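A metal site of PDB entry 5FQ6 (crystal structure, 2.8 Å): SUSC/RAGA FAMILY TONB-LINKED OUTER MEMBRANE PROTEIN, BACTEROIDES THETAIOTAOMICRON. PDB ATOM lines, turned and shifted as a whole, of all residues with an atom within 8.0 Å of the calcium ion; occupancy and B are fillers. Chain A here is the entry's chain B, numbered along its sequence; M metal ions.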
ATOM      1  N   PRO A  80      19.403 -12.868  -0.567  1.00  0.00           N
ATOM      2  CA  PRO A  80      18.301 -13.795  -0.813  1.00  0.00           C
ATOM      3  C   PRO A  80      17.338 -13.275  -1.873  1.00  0.00           C
ATOM      4  O   PRO A  80      16.932 -12.105  -1.873  1.00  0.00           O
ATOM      5  CB  PRO A  80      17.643 -13.909   0.563  1.00  0.00           C
ATOM      6  CG  PRO A  80      18.761 -13.583   1.538  1.00  0.00           C
ATOM      7  CD  PRO A  80      19.519 -12.499   0.851  1.00  0.00           C
ATOM      8  N   SER A 186      24.181 -19.171   6.433  1.00  0.00           N
ATOM      9  CA  SER A 186      25.053 -18.382   5.579  1.00  0.00           C
ATOM     10  C   SER A 186      25.886 -17.440   6.436  1.00  0.00           C
ATOM     11  O   SER A 186      25.365 -16.826   7.374  1.00  0.00           O
ATOM     12  CB  SER A 186      24.244 -17.613   4.526  1.00  0.00           C
ATOM     13  OG  SER A 186      23.523 -16.529   5.091  1.00  0.00           O
ATOM     14  N   PHE A 249      28.180  -8.609  10.829  1.00  0.00           N
ATOM     15  CA  PHE A 249      27.292  -9.558  10.177  1.00  0.00           C
ATOM     16  C   PHE A 249      26.859 -10.661  11.146  1.00  0.00           C
ATOM     17  O   PHE A 249      27.683 -11.211  11.881  1.00  0.00           O
ATOM     18  CB  PHE A 249      27.976 -10.145   8.947  1.00  0.00           C
ATOM     19  CG  PHE A 249      28.389  -9.114   7.935  1.00  0.00           C
ATOM     20  CD1 PHE A 249      27.498  -8.662   6.973  1.00  0.00           C
ATOM     21  CD2 PHE A 249      29.671  -8.585   7.941  1.00  0.00           C
ATOM     22  CE1 PHE A 249      27.873  -7.720   6.021  1.00  0.00           C
ATOM     23  CE2 PHE A 249      30.045  -7.643   6.989  1.00  0.00           C
ATOM     24  CZ  PHE A 249      29.143  -7.209   6.035  1.00  0.00           C
ATOM     25  N   ASP A 250      25.560 -10.940  11.156  1.00  0.00           N
ATOM     26  CA  ASP A 250      25.005 -12.092  11.855  1.00  0.00           C
ATOM     27  C   ASP A 250      25.250 -13.328  10.977  1.00  0.00           C
ATOM     28  O   ASP A 250      25.963 -13.273   9.973  1.00  0.00           O
ATOM     29  CB  ASP A 250      23.513 -11.859  12.143  1.00  0.00           C
ATOM     30  CG  ASP A 250      23.265 -10.662  13.066  1.00  0.00           C
ATOM     31  OD1 ASP A 250      23.980 -10.537  14.089  1.00  0.00           O
ATOM     32  OD2 ASP A 250      22.340  -9.862  12.796  1.00  0.00           O
ATOM     33  N   ALA A 251      24.643 -14.453  11.349  1.00  0.00           N
ATOM     34  CA  ALA A 251      24.634 -15.634  10.495  1.00  0.00           C
ATOM     35  C   ALA A 251      23.257 -15.750   9.858  1.00  0.00           C
ATOM     36  O   ALA A 251      22.242 -15.712  10.551  1.00  0.00           O
ATOM     37  CB  ALA A 251      24.969 -16.890  11.298  1.00  0.00           C
ATOM     38  N   GLY A 252      23.226 -15.856   8.524  1.00  0.00           N
ATOM     39  CA  GLY A 252      21.957 -16.048   7.841  1.00  0.00           C
ATOM     40  C   GLY A 252      21.357 -17.422   8.127  1.00  0.00           C
ATOM     41  O   GLY A 252      22.069 -18.393   8.345  1.00  0.00           O
ATOM     42  N   PHE A 253      20.022 -17.488   8.147  1.00  0.00           N
ATOM     43  CA  PHE A 253      19.310 -18.738   8.397  1.00  0.00           C
ATOM     44  C   PHE A 253      18.179 -18.866   7.383  1.00  0.00           C
ATOM     45  O   PHE A 253      17.468 -17.906   7.121  1.00  0.00           O
ATOM     46  CB  PHE A 253      18.756 -18.812   9.825  1.00  0.00           C
ATOM     47  CG  PHE A 253      18.103 -20.134  10.184  1.00  0.00           C
ATOM     48  CD1 PHE A 253      18.224 -21.256   9.372  1.00  0.00           C
ATOM     49  CD2 PHE A 253      17.340 -20.249  11.339  1.00  0.00           C
ATOM     50  CE1 PHE A 253      17.587 -22.445   9.694  1.00  0.00           C
ATOM     51  CE2 PHE A 253      16.705 -21.439  11.671  1.00  0.00           C
ATOM     52  CZ  PHE A 253      16.828 -22.536  10.843  1.00  0.00           C
ATOM     53  N   ASP A 279      14.121 -17.295   3.900  1.00  0.00           N
ATOM     54  CA  ASP A 279      15.530 -16.936   4.055  1.00  0.00           C
ATOM     55  C   ASP A 279      15.673 -15.551   4.659  1.00  0.00           C
ATOM     56  O   ASP A 279      15.060 -14.594   4.183  1.00  0.00           O
ATOM     57  CB  ASP A 279      16.246 -16.991   2.705  1.00  0.00           C
ATOM     58  CG  ASP A 279      17.745 -17.232   2.840  1.00  0.00           C
ATOM     59  OD1 ASP A 279      18.264 -17.186   3.984  1.00  0.00           O
ATOM     60  OD2 ASP A 279      18.391 -17.459   1.808  1.00  0.00           O
ATOM     61  N   ASP A 280      16.521 -15.446   5.686  1.00  0.00           N
ATOM     62  CA  ASP A 280      16.917 -14.184   6.304  1.00  0.00           C
ATOM     63  C   ASP A 280      18.447 -14.145   6.368  1.00  0.00           C
ATOM     64  O   ASP A 280      19.036 -14.807   7.234  1.00  0.00           O
ATOM     65  CB  ASP A 280      16.295 -14.068   7.702  1.00  0.00           C
ATOM     66  CG  ASP A 280      16.539 -12.704   8.337  1.00  0.00           C
ATOM     67  OD1 ASP A 280      17.584 -12.073   8.042  1.00  0.00           O
ATOM     68  OD2 ASP A 280      15.671 -12.274   9.139  1.00  0.00           O
ATOM     69  N   GLY A 281      19.078 -13.334   5.500  1.00  0.00           N
ATOM     70  CA  GLY A 281      20.524 -13.363   5.294  1.00  0.00           C
ATOM     71  C   GLY A 281      21.375 -12.743   6.421  1.00  0.00           C
ATOM     72  O   GLY A 281      20.876 -12.258   7.421  1.00  0.00           O
ATOM     73  N   MET A 282      22.700 -12.746   6.191  1.00  0.00           N
ATOM     74  CA  MET A 282      23.735 -12.418   7.192  1.00  0.00           C
ATOM     75  C   MET A 282      23.820 -10.942   7.567  1.00  0.00           C
ATOM     76  O   MET A 282      24.488 -10.617   8.558  1.00  0.00           O
ATOM     77  CB  MET A 282      25.141 -12.814   6.697  1.00  0.00           C
ATOM     78  CG  MET A 282      25.201 -13.332   5.289  1.00  0.00           C
ATOM     79  SD  MET A 282      26.782 -12.891   4.591  1.00  0.00           S
ATOM     80  CE  MET A 282      26.315 -11.424   3.680  1.00  0.00           C
ATOM     81  N   ILE A 283      23.200 -10.051   6.807  1.00  0.00           N
ATOM     82  CA  ILE A 283      23.109  -8.637   7.210  1.00  0.00           C
ATOM     83  C   ILE A 283      22.178  -8.535   8.410  1.00  0.00           C
ATOM     84  O   ILE A 283      21.070  -9.116   8.373  1.00  0.00           O
ATOM     85  CB  ILE A 283      22.598  -7.797   6.037  1.00  0.00           C
ATOM     86  CG1 ILE A 283      23.538  -7.986   4.837  1.00  0.00           C
ATOM     87  CG2 ILE A 283      22.473  -6.329   6.446  1.00  0.00           C
ATOM     88  CD1 ILE A 283      23.044  -7.376   3.560  1.00  0.00           C
ATOM     89  N   PRO A 284      22.542  -7.813   9.477  1.00  0.00           N
ATOM     90  CA  PRO A 284      21.651  -7.729  10.645  1.00  0.00           C
ATOM     91  C   PRO A 284      20.288  -7.191  10.239  1.00  0.00           C
ATOM     92  O   PRO A 284      20.155  -6.485   9.232  1.00  0.00           O
ATOM     93  CB  PRO A 284      22.386  -6.763  11.586  1.00  0.00           C
ATOM     94  CG  PRO A 284      23.773  -6.655  11.079  1.00  0.00           C
ATOM     95  CD  PRO A 284      23.692  -6.905   9.597  1.00  0.00           C
ATOM     96  N   THR A 285      19.284  -7.551  11.052  1.00  0.00           N
ATOM     97  CA  THR A 285      17.847  -7.355  10.814  1.00  0.00           C
ATOM     98  C   THR A 285      17.315  -8.218   9.673  1.00  0.00           C
ATOM     99  O   THR A 285      18.043  -9.015   9.065  1.00  0.00           O
ATOM    100  CB  THR A 285      17.467  -5.887  10.531  1.00  0.00           C
ATOM    101  OG1 THR A 285      17.912  -5.479   9.235  1.00  0.00           O
ATOM    102  CG2 THR A 285      18.031  -4.954  11.599  1.00  0.00           C
ATOM    103  N   ASP A 286      16.025  -8.039   9.396  1.00  0.00           N
ATOM    104  CA  ASP A 286      15.285  -8.787   8.389  1.00  0.00           C
ATOM    105  C   ASP A 286      15.293  -8.086   7.033  1.00  0.00           C
ATOM    106  O   ASP A 286      14.434  -8.364   6.189  1.00  0.00           O
ATOM    107  CB  ASP A 286      13.847  -8.993   8.863  1.00  0.00           C
ATOM    108  CG  ASP A 286      13.079  -7.693   8.943  1.00  0.00           C
ATOM    109  OD1 ASP A 286      13.511  -6.756   9.661  1.00  0.00           O
ATOM    110  OD2 ASP A 286      12.031  -7.598   8.253  1.00  0.00           O
ATOM    111  N   ALA A 287      16.249  -7.187   6.812  1.00  0.00           N
ATOM    112  CA  ALA A 287      16.211  -6.403   5.586  1.00  0.00           C
ATOM    113  C   ALA A 287      16.587  -7.241   4.376  1.00  0.00           C
ATOM    114  O   ALA A 287      16.269  -6.869   3.246  1.00  0.00           O
ATOM    115  CB  ALA A 287      17.147  -5.197   5.735  1.00  0.00           C
ATOM    116  N   ASP A 288      17.282  -8.358   4.618  1.00  0.00           N
ATOM    117  CA  ASP A 288      17.692  -9.289   3.569  1.00  0.00           C
ATOM    118  C   ASP A 288      16.822 -10.531   3.733  1.00  0.00           C
ATOM    119  O   ASP A 288      17.160 -11.457   4.461  1.00  0.00           O
ATOM    120  CB  ASP A 288      19.182  -9.600   3.690  1.00  0.00           C
ATOM    121  CG  ASP A 288      19.633  -9.988   5.126  1.00  0.00           C
ATOM    122  OD1 ASP A 288      18.815 -10.057   6.093  1.00  0.00           O
ATOM    123  OD2 ASP A 288      20.869 -10.216   5.247  1.00  0.00           O
ATOM    124  N   SER A 289      15.670 -10.521   3.063  1.00  0.00           N
ATOM    125  CA  SER A 289      14.675 -11.555   3.263  1.00  0.00           C
ATOM    126  C   SER A 289      14.092 -12.007   1.929  1.00  0.00           C
ATOM    127  O   SER A 289      13.974 -11.227   0.986  1.00  0.00           O
ATOM    128  CB  SER A 289      13.566 -11.088   4.209  1.00  0.00           C
ATOM    129  OG  SER A 289      14.072 -11.003   5.530  1.00  0.00           O
ATOM    130  N   LEU A 372      19.109   0.111   8.184  1.00  0.00           N
ATOM    131  CA  LEU A 372      18.443  -1.178   8.043  1.00  0.00           C
ATOM    132  C   LEU A 372      17.107  -1.252   8.767  1.00  0.00           C
ATOM    133  O   LEU A 372      16.229  -2.016   8.361  1.00  0.00           O
ATOM    134  CB  LEU A 372      19.340  -2.301   8.570  1.00  0.00           C
ATOM    135  CG  LEU A 372      20.603  -2.621   7.795  1.00  0.00           C
ATOM    136  CD1 LEU A 372      21.471  -3.505   8.637  1.00  0.00           C
ATOM    137  CD2 LEU A 372      20.255  -3.287   6.488  1.00  0.00           C
HETATM  138 CA    CA M   1      19.385 -10.854   8.406  1.00  0.00          CA
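The calcium ion is bound by OD1 of Asp 280, at 2.2 Å. The calcium ion is bound by the backbone carbonyl oxygen (O) of Gly 281. The calcium ion is bound by O of Thr 285, 2.4 Å away. The calcium ion is bound by O of Ile 283. OD1 of Asp 288 binds the calcium ion (2.5 Å).
The backbone carbonyl oxygen of Asp 280 is in hydrogen-bond range of the backbone NH of Phe 253 (3.0 Å). The side-chain hydroxyl (OG1) of Thr 285 sits close to the backbone NH (N) of Ala 287, 3.4 Å away. The side-chain carboxylate of Asp 288 sits at hydrogen-bond distance from the backbone NH of Met 282, 3.3 Å away.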
